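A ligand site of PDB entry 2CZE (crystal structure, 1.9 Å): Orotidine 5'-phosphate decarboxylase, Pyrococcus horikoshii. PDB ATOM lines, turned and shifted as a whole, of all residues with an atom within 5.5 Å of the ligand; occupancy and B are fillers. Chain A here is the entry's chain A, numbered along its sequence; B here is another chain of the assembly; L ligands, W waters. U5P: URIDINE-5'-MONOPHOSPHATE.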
ATOM      1  N   ALA A   5     -27.866  24.371 -12.995  1.00  0.00           N
ATOM      2  CA  ALA A   5     -28.499  23.119 -12.602  1.00  0.00           C
ATOM      3  C   ALA A   5     -29.521  23.457 -11.536  1.00  0.00           C
ATOM      4  O   ALA A   5     -29.167  23.664 -10.377  1.00  0.00           O
ATOM      5  CB  ALA A   5     -27.469  22.150 -12.071  1.00  0.00           C
ATOM      6  N   ASP A   7     -31.671  22.316  -9.164  1.00  0.00           N
ATOM      7  CA  ASP A   7     -32.095  21.176  -8.371  1.00  0.00           C
ATOM      8  C   ASP A   7     -32.875  21.528  -7.108  1.00  0.00           C
ATOM      9  O   ASP A   7     -32.494  21.143  -6.012  1.00  0.00           O
ATOM     10  CB  ASP A   7     -30.876  20.302  -8.038  1.00  0.00           C
ATOM     11  CG  ASP A   7     -30.193  19.767  -9.277  1.00  0.00           C
ATOM     12  OD1 ASP A   7     -30.926  19.323 -10.204  1.00  0.00           O
ATOM     13  OD2 ASP A   7     -28.944  19.787  -9.334  1.00  0.00           O
ATOM     14  N   LYS A  29     -30.285  23.269 -16.735  1.00  0.00           N
ATOM     15  CA  LYS A  29     -30.319  21.803 -16.649  1.00  0.00           C
ATOM     16  C   LYS A  29     -31.312  21.406 -15.564  1.00  0.00           C
ATOM     17  O   LYS A  29     -31.199  21.863 -14.422  1.00  0.00           O
ATOM     18  CB  LYS A  29     -28.932  21.252 -16.290  1.00  0.00           C
ATOM     19  CG  LYS A  29     -28.840  19.717 -16.319  1.00  0.00           C
ATOM     20  CD  LYS A  29     -27.429  19.192 -16.039  1.00  0.00           C
ATOM     21  CE  LYS A  29     -27.086  19.240 -14.540  1.00  0.00           C
ATOM     22  NZ  LYS A  29     -27.901  18.279 -13.731  1.00  0.00           N
ATOM     23  N   ASN A  31     -33.222  18.217 -13.413  1.00  0.00           N
ATOM     24  CA  ASN A  31     -32.945  16.844 -13.030  1.00  0.00           C
ATOM     25  C   ASN A  31     -34.235  16.322 -12.373  1.00  0.00           C
ATOM     26  O   ASN A  31     -35.233  17.041 -12.314  1.00  0.00           O
ATOM     27  CB  ASN A  31     -31.764  16.824 -12.033  1.00  0.00           C
ATOM     28  CG  ASN A  31     -31.018  15.486 -11.984  1.00  0.00           C
ATOM     29  OD1 ASN A  31     -31.625  14.410 -12.035  1.00  0.00           O
ATOM     30  ND2 ASN A  31     -29.693  15.566 -11.842  1.00  0.00           N
ATOM     31  N   ASP A  57     -31.412  16.304 -17.364  1.00  0.00           N
ATOM     32  CA  ASP A  57     -30.374  15.399 -16.852  1.00  0.00           C
ATOM     33  C   ASP A  57     -31.096  14.242 -16.172  1.00  0.00           C
ATOM     34  O   ASP A  57     -31.282  14.240 -14.958  1.00  0.00           O
ATOM     35  CB  ASP A  57     -29.487  16.138 -15.833  1.00  0.00           C
ATOM     36  CG  ASP A  57     -28.255  15.338 -15.422  1.00  0.00           C
ATOM     37  OD1 ASP A  57     -28.080  14.195 -15.928  1.00  0.00           O
ATOM     38  OD2 ASP A  57     -27.452  15.840 -14.605  1.00  0.00           O
ATOM     39  N   LYS A  59     -30.158  10.933 -16.659  1.00  0.00           N
ATOM     40  CA  LYS A  59     -29.230   9.831 -16.414  1.00  0.00           C
ATOM     41  C   LYS A  59     -29.946   8.549 -16.786  1.00  0.00           C
ATOM     42  O   LYS A  59     -29.870   7.569 -16.056  1.00  0.00           O
ATOM     43  CB  LYS A  59     -28.838   9.763 -14.933  1.00  0.00           C
ATOM     44  CG  LYS A  59     -28.010  10.941 -14.423  1.00  0.00           C
ATOM     45  CD  LYS A  59     -26.612  10.898 -15.025  1.00  0.00           C
ATOM     46  CE  LYS A  59     -25.695  11.868 -14.325  1.00  0.00           C
ATOM     47  NZ  LYS A  59     -26.230  13.259 -14.413  1.00  0.00           N
ATOM     48  N   GLU A 107     -17.504  10.241 -17.765  1.00  0.00           N
ATOM     49  CA  GLU A 107     -16.894  10.084 -16.441  1.00  0.00           C
ATOM     50  C   GLU A 107     -17.588  11.044 -15.482  1.00  0.00           C
ATOM     51  O   GLU A 107     -17.705  12.233 -15.773  1.00  0.00           O
ATOM     52  CB  GLU A 107     -15.391  10.358 -16.466  1.00  0.00           C
ATOM     53  CG  GLU A 107     -14.790  10.296 -15.074  1.00  0.00           C
ATOM     54  CD  GLU A 107     -13.268  10.254 -15.054  1.00  0.00           C
ATOM     55  OE1 GLU A 107     -12.703  10.469 -13.961  1.00  0.00           O
ATOM     56  OE2 GLU A 107     -12.648   9.998 -16.117  1.00  0.00           O
ATOM     57  N   MET A 108     -18.038  10.542 -14.320  1.00  0.00           N
ATOM     58  CA  MET A 108     -18.753  11.390 -13.364  1.00  0.00           C
ATOM     59  C   MET A 108     -17.841  12.098 -12.365  1.00  0.00           C
ATOM     60  O   MET A 108     -16.681  11.738 -12.214  1.00  0.00           O
ATOM     61  CB  MET A 108     -19.836  10.568 -12.654  1.00  0.00           C
ATOM     62  CG  MET A 108     -20.959  10.122 -13.583  1.00  0.00           C
ATOM     63  SD  MET A 108     -22.232   9.115 -12.764  1.00  0.00           S
ATOM     64  CE  MET A 108     -23.149  10.400 -11.839  1.00  0.00           C
ATOM     65  N   SER A 109     -18.378  13.100 -11.674  1.00  0.00           N
ATOM     66  CA  SER A 109     -17.597  13.931 -10.767  1.00  0.00           C
ATOM     67  C   SER A 109     -17.419  13.529  -9.313  1.00  0.00           C
ATOM     68  O   SER A 109     -16.547  14.057  -8.629  1.00  0.00           O
ATOM     69  CB  SER A 109     -18.154  15.349 -10.776  1.00  0.00           C
ATOM     70  OG  SER A 109     -19.490  15.343 -10.307  1.00  0.00           O
ATOM     71  N   HIS A 110     -18.254  12.600  -8.835  1.00  0.00           N
ATOM     72  CA  HIS A 110     -18.204  12.200  -7.422  1.00  0.00           C
ATOM     73  C   HIS A 110     -17.184  11.084  -7.150  1.00  0.00           C
ATOM     74  O   HIS A 110     -16.722  10.414  -8.078  1.00  0.00           O
ATOM     75  CB  HIS A 110     -19.609  11.752  -6.970  1.00  0.00           C
ATOM     76  CG  HIS A 110     -20.100  10.532  -7.693  1.00  0.00           C
ATOM     77  ND1 HIS A 110     -20.268  10.483  -9.065  1.00  0.00           N
ATOM     78  CD2 HIS A 110     -20.429   9.295  -7.246  1.00  0.00           C
ATOM     79  CE1 HIS A 110     -20.683   9.285  -9.423  1.00  0.00           C
ATOM     80  NE2 HIS A 110     -20.786   8.538  -8.335  1.00  0.00           N
ATOM     81  N   ILE A 137     -20.525  14.058 -20.629  1.00  0.00           N
ATOM     82  CA  ILE A 137     -20.278  14.517 -19.276  1.00  0.00           C
ATOM     83  C   ILE A 137     -18.853  14.130 -18.885  1.00  0.00           C
ATOM     84  O   ILE A 137     -18.469  12.967 -19.017  1.00  0.00           O
ATOM     85  CB  ILE A 137     -21.244  13.862 -18.255  1.00  0.00           C
ATOM     86  CG1 ILE A 137     -22.669  14.349 -18.502  1.00  0.00           C
ATOM     87  CG2 ILE A 137     -20.814  14.203 -16.812  1.00  0.00           C
ATOM     88  CD1 ILE A 137     -22.826  15.857 -18.435  1.00  0.00           C
ATOM     89  N   PRO A 162     -19.882  19.089 -14.833  1.00  0.00           N
ATOM     90  CA  PRO A 162     -20.577  19.405 -13.579  1.00  0.00           C
ATOM     91  C   PRO A 162     -19.523  19.219 -12.483  1.00  0.00           C
ATOM     92  O   PRO A 162     -18.407  18.773 -12.776  1.00  0.00           O
ATOM     93  CB  PRO A 162     -21.685  18.366 -13.523  1.00  0.00           C
ATOM     94  CG  PRO A 162     -21.027  17.164 -14.144  1.00  0.00           C
ATOM     95  CD  PRO A 162     -20.256  17.745 -15.320  1.00  0.00           C
ATOM     96  N   GLY A 163     -19.843  19.552 -11.239  1.00  0.00           N
ATOM     97  CA  GLY A 163     -18.874  19.422 -10.167  1.00  0.00           C
ATOM     98  C   GLY A 163     -18.110  20.715  -9.912  1.00  0.00           C
ATOM     99  O   GLY A 163     -17.051  20.712  -9.289  1.00  0.00           O
ATOM    100  N   ILE A 164     -18.655  21.826 -10.411  1.00  0.00           N
ATOM    101  CA  ILE A 164     -18.059  23.141 -10.247  1.00  0.00           C
ATOM    102  C   ILE A 164     -18.708  23.864  -9.067  1.00  0.00           C
ATOM    103  O   ILE A 164     -19.925  23.987  -9.014  1.00  0.00           O
ATOM    104  CB  ILE A 164     -18.259  23.992 -11.521  1.00  0.00           C
ATOM    105  CG1 ILE A 164     -17.689  23.253 -12.743  1.00  0.00           C
ATOM    106  CG2 ILE A 164     -17.583  25.362 -11.343  1.00  0.00           C
ATOM    107  CD1 ILE A 164     -16.194  22.967 -12.679  1.00  0.00           C
ATOM    108  N   ALA A 166     -19.799  23.735  -5.479  1.00  0.00           N
ATOM    109  CA  ALA A 166     -20.072  22.901  -4.320  1.00  0.00           C
ATOM    110  C   ALA A 166     -19.151  21.676  -4.240  1.00  0.00           C
ATOM    111  O   ALA A 166     -18.591  21.368  -3.179  1.00  0.00           O
ATOM    112  CB  ALA A 166     -21.543  22.443  -4.347  1.00  0.00           C
ATOM    113  N   GLN A 167     -18.985  20.950  -5.336  1.00  0.00           N
ATOM    114  CA  GLN A 167     -18.137  19.765  -5.289  1.00  0.00           C
ATOM    115  C   GLN A 167     -16.629  20.060  -5.301  1.00  0.00           C
ATOM    116  O   GLN A 167     -15.813  19.134  -5.234  1.00  0.00           O
ATOM    117  CB  GLN A 167     -18.489  18.821  -6.440  1.00  0.00           C
ATOM    118  CG  GLN A 167     -19.919  18.282  -6.323  1.00  0.00           C
ATOM    119  CD  GLN A 167     -20.295  17.442  -7.508  1.00  0.00           C
ATOM    120  OE1 GLN A 167     -19.644  16.442  -7.807  1.00  0.00           O
ATOM    121  NE2 GLN A 167     -21.362  17.847  -8.204  1.00  0.00           N
ATOM    122  N   ILE A 183     -21.314  23.327 -15.753  1.00  0.00           N
ATOM    123  CA  ILE A 183     -22.558  23.110 -15.035  1.00  0.00           C
ATOM    124  C   ILE A 183     -22.402  23.553 -13.592  1.00  0.00           C
ATOM    125  O   ILE A 183     -21.470  23.153 -12.901  1.00  0.00           O
ATOM    126  CB  ILE A 183     -22.961  21.637 -15.096  1.00  0.00           C
ATOM    127  CG1 ILE A 183     -23.220  21.246 -16.565  1.00  0.00           C
ATOM    128  CG2 ILE A 183     -24.206  21.386 -14.248  1.00  0.00           C
ATOM    129  CD1 ILE A 183     -23.292  19.734 -16.780  1.00  0.00           C
ATOM    130  N   VAL A 184     -23.312  24.405 -13.137  1.00  0.00           N
ATOM    131  CA  VAL A 184     -23.241  24.911 -11.767  1.00  0.00           C
ATOM    132  C   VAL A 184     -24.613  24.870 -11.141  1.00  0.00           C
ATOM    133  O   VAL A 184     -25.562  25.429 -11.683  1.00  0.00           O
ATOM    134  CB  VAL A 184     -22.717  26.378 -11.718  1.00  0.00           C
ATOM    135  CG1 VAL A 184     -22.631  26.845 -10.268  1.00  0.00           C
ATOM    136  CG2 VAL A 184     -21.326  26.447 -12.365  1.00  0.00           C
ATOM    137  N   GLY A 185     -24.700  24.218  -9.983  1.00  0.00           N
ATOM    138  CA  GLY A 185     -25.951  24.110  -9.274  1.00  0.00           C
ATOM    139  C   GLY A 185     -25.960  24.887  -7.973  1.00  0.00           C
ATOM    140  O   GLY A 185     -26.191  26.105  -7.974  1.00  0.00           O
ATOM    141  N   ARG A 186     -25.688  24.204  -6.869  1.00  0.00           N
ATOM    142  CA  ARG A 186     -25.707  24.813  -5.540  1.00  0.00           C
ATOM    143  C   ARG A 186     -24.986  26.146  -5.388  1.00  0.00           C
ATOM    144  O   ARG A 186     -25.486  27.048  -4.705  1.00  0.00           O
ATOM    145  CB  ARG A 186     -25.191  23.811  -4.494  1.00  0.00           C
ATOM    146  CG  ARG A 186     -26.188  22.644  -4.255  1.00  0.00           C
ATOM    147  CD  ARG A 186     -25.549  21.474  -3.490  1.00  0.00           C
ATOM    148  NE  ARG A 186     -24.698  20.682  -4.376  1.00  0.00           N
ATOM    149  CZ  ARG A 186     -23.967  19.649  -3.985  1.00  0.00           C
ATOM    150  NH1 ARG A 186     -23.974  19.275  -2.711  1.00  0.00           N
ATOM    151  NH2 ARG A 186     -23.259  18.968  -4.870  1.00  0.00           N
ATOM    152  N   ALA A 187     -23.810  26.293  -6.014  1.00  0.00           N
ATOM    153  CA  ALA A 187     -23.065  27.546  -5.896  1.00  0.00           C
ATOM    154  C   ALA A 187     -23.899  28.737  -6.380  1.00  0.00           C
ATOM    155  O   ALA A 187     -23.636  29.881  -6.007  1.00  0.00           O
ATOM    156  CB  ALA A 187     -21.746  27.485  -6.678  1.00  0.00           C
ATOM    157  N   TYR A 189     -27.833  28.427  -7.026  1.00  0.00           N
ATOM    158  CA  TYR A 189     -29.158  28.401  -6.413  1.00  0.00           C
ATOM    159  C   TYR A 189     -29.243  28.410  -4.886  1.00  0.00           C
ATOM    160  O   TYR A 189     -30.289  28.730  -4.325  1.00  0.00           O
ATOM    161  CB  TYR A 189     -30.000  27.266  -7.016  1.00  0.00           C
ATOM    162  CG  TYR A 189     -29.697  25.856  -6.582  1.00  0.00           C
ATOM    163  CD1 TYR A 189     -30.016  25.412  -5.289  1.00  0.00           C
ATOM    164  CD2 TYR A 189     -29.158  24.931  -7.480  1.00  0.00           C
ATOM    165  CE1 TYR A 189     -29.799  24.091  -4.891  1.00  0.00           C
ATOM    166  CE2 TYR A 189     -28.933  23.608  -7.097  1.00  0.00           C
ATOM    167  CZ  TYR A 189     -29.258  23.191  -5.813  1.00  0.00           C
ATOM    168  OH  TYR A 189     -29.046  21.870  -5.459  1.00  0.00           O
ATOM    169  N   ASP B  62     -27.078   8.875 -10.026  1.00  0.00           N
ATOM    170  CA  ASP B  62     -26.536  10.226  -9.924  1.00  0.00           C
ATOM    171  C   ASP B  62     -25.553  10.287  -8.763  1.00  0.00           C
ATOM    172  O   ASP B  62     -25.299   9.270  -8.114  1.00  0.00           O
ATOM    173  CB  ASP B  62     -27.658  11.240  -9.682  1.00  0.00           C
ATOM    174  CG  ASP B  62     -27.425  12.567 -10.395  1.00  0.00           C
ATOM    175  OD1 ASP B  62     -26.311  13.144 -10.306  1.00  0.00           O
ATOM    176  OD2 ASP B  62     -28.385  13.041 -11.048  1.00  0.00           O
ATOM    177  N   ILE B  63     -24.994  11.475  -8.519  1.00  0.00           N
ATOM    178  CA  ILE B  63     -24.067  11.669  -7.403  1.00  0.00           C
ATOM    179  C   ILE B  63     -24.848  11.528  -6.107  1.00  0.00           C
ATOM    180  O   ILE B  63     -26.080  11.620  -6.093  1.00  0.00           O
ATOM    181  CB  ILE B  63     -23.404  13.065  -7.440  1.00  0.00           C
ATOM    182  CG1 ILE B  63     -24.458  14.152  -7.187  1.00  0.00           C
ATOM    183  CG2 ILE B  63     -22.736  13.282  -8.815  1.00  0.00           C
ATOM    184  CD1 ILE B  63     -23.846  15.533  -7.115  1.00  0.00           C
ATOM    185  N   THR B  66     -27.632  14.319  -5.178  1.00  0.00           N
ATOM    186  CA  THR B  66     -28.832  14.290  -5.984  1.00  0.00           C
ATOM    187  C   THR B  66     -29.649  13.030  -5.745  1.00  0.00           C
ATOM    188  O   THR B  66     -30.888  13.077  -5.721  1.00  0.00           O
ATOM    189  CB  THR B  66     -28.494  14.415  -7.475  1.00  0.00           C
ATOM    190  OG1 THR B  66     -27.752  15.638  -7.680  1.00  0.00           O
ATOM    191  CG2 THR B  66     -29.755  14.474  -8.293  1.00  0.00           C
HETATM  192  N1  U5P L   1     -24.196  15.818 -12.057  1.00  0.00           N
HETATM  193  C2  U5P L   1     -23.019  15.888 -11.293  1.00  0.00           C
HETATM  194  N3  U5P L   1     -21.943  15.041 -11.621  1.00  0.00           N
HETATM  195  C4  U5P L   1     -22.045  14.152 -12.690  1.00  0.00           C
HETATM  196  C5  U5P L   1     -23.216  14.072 -13.440  1.00  0.00           C
HETATM  197  C6  U5P L   1     -24.287  14.910 -13.122  1.00  0.00           C
HETATM  198  O2  U5P L   1     -22.904  16.658 -10.342  1.00  0.00           O
HETATM  199  O4  U5P L   1     -21.082  13.435 -12.980  1.00  0.00           O
HETATM  200  C1' U5P L   1     -25.309  16.759 -11.811  1.00  0.00           C
HETATM  201  C2' U5P L   1     -25.803  16.748 -10.351  1.00  0.00           C
HETATM  202  O2' U5P L   1     -26.828  15.760 -10.222  1.00  0.00           O
HETATM  203  C3' U5P L   1     -26.434  18.140 -10.272  1.00  0.00           C
HETATM  204  C4' U5P L   1     -25.430  18.968 -11.068  1.00  0.00           C
HETATM  205  O3' U5P L   1     -27.717  18.163 -10.904  1.00  0.00           O
HETATM  206  O4' U5P L   1     -24.869  18.103 -12.059  1.00  0.00           O
HETATM  207  C5' U5P L   1     -24.300  19.458 -10.149  1.00  0.00           C
HETATM  208  O5' U5P L   1     -24.860  20.364  -9.199  1.00  0.00           O
HETATM  209  P   U5P L   1     -23.985  21.088  -8.053  1.00  0.00           P
HETATM  210  O1P U5P L   1     -24.878  21.581  -6.978  1.00  0.00           O
HETATM  211  O2P U5P L   1     -23.159  22.254  -8.779  1.00  0.00           O
HETATM  212  O3P U5P L   1     -22.919  20.015  -7.516  1.00  0.00           O
HETATM  213  O   HOH W   1     -22.159  24.241  -7.404  1.00  0.00           O
HETATM  214  O   HOH W   2     -27.514  20.380  -7.119  1.00  0.00           O
HETATM  215  O   HOH W   3     -20.404  21.212  -7.695  1.00  0.00           O
HETATM  216  O   HOH W   4     -21.655  21.490 -10.767  1.00  0.00           O
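The side-chain hydroxyl (OG) of Ser 109 is in hydrogen-bond range of the side-chain amide oxygen (OE1) of Gln 167.
The side-chain carboxylate of Asp 57 lies within salt-bridge range of the side-chain amino group of Lys 59 (2.6 Å).
The backbone carbonyl oxygen (O) of Val 184 lies within hydrogen-bond range of the backbone NH (N) of Ala 5, at 2.9 Å.
N of Glu 107 sits at hydrogen-bond distance from O of Ile 137 (3.2 Å).
OD1 of Asn 31 lies close to O of Asp 57, 2.9 Å away.
ND2 of Asn 31 lies within hydrogen-bond range of OD2 of Asp 62 of chain B (3.0 Å).
OD2 of Asp 57 lies within salt-bridge range of NZ of Lys 29 (2.6 Å).
OD1 of Asp 62 of chain B is in hydrogen-bond range of O2' of the ligand, at 2.7 Å.
OG of Ser 109 sits at hydrogen-bond distance from N3 of the ligand.
OD2 of Asp 7 is in hydrogen-bond range of O3' of the ligand (2.6 Å).
An oxygen (O1P) of the ligand lies within salt-bridge range of the guanidinium group of Arg 186 (2.8 Å).
An oxygen (O3P) of the ligand lies within hydrogen-bond range of the side-chain amide nitrogen (NE2) of Gln 167 (2.8 Å).
N of Arg 186 lies within hydrogen-bond range of O1P of the ligand, 2.7 Å away.
The side-chain hydroxyl of Thr 66 of chain B is in hydrogen-bond range of an oxygen (O2') of the ligand (2.7 Å).
An oxygen (O4) of the ligand is in hydrogen-bond range of the backbone NH (N) of Ser 109.
The backbone NH of Gly 185 is in hydrogen-bond range of an oxygen (O2P) of the ligand (2.8 Å).
NZ of Lys 29 is in hydrogen-bond range of O3' of the ligand, 2.8 Å away.
The side-chain amide nitrogen of Asn 31 is in hydrogen-bond range of an oxygen (O2') of the ligand (3.3 Å).
Water W4 lies within hydrogen-bond range of an oxygen (O2P) of the ligand, the backbone NH (N) of Gly 163, the backbone carbonyl oxygen (O) of Ile 183 and the backbone NH (N) of Ile 164.
Water W1 lies within hydrogen-bond range of an oxygen (O2P) of the ligand (2.6 Å), the backbone carbonyl oxygen (O) of Ile 164 (2.8 Å), the backbone NH (N) of Ala 187 (3.0 Å) and the backbone NH (N) of Ala 166 (3.1 Å).
Water W3 lies within hydrogen-bond range of the backbone NH of Gln 167 (2.8 Å), an oxygen (O3P) of the ligand (2.8 Å), the backbone carbonyl oxygen of Ile 164 (3.1 Å) and the backbone NH of Ala 166 (3.4 Å).
Water W2 lies within hydrogen-bond range of the side-chain carboxylate (OD2) of Asp 7 (2.7 Å), the side-chain hydroxyl (OH) of Tyr 189 (2.7 Å) and an oxygen (O1P) of the ligand (2.9 Å).
Merely in contact with the ligand: Ala 5 (3.9 Å), Asp 57 (3.6 Å), Lys 59 (2.9 Å), Met 108 (3.1 Å), Ile 137 (3.9 Å), Pro 162 (3.4 Å), Ile 164 (3.7 Å), Val 184 (3.8 Å) and Ile 63 of chain B (3.4 Å).
Hydrophobic or aromatic side chains that line the ligand: Ala 5, Met 108, Ile 137, Pro 162 and Ile 63 of chain B.
Of the 25 residues printed, 18 come within 4 Å of the ligand.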
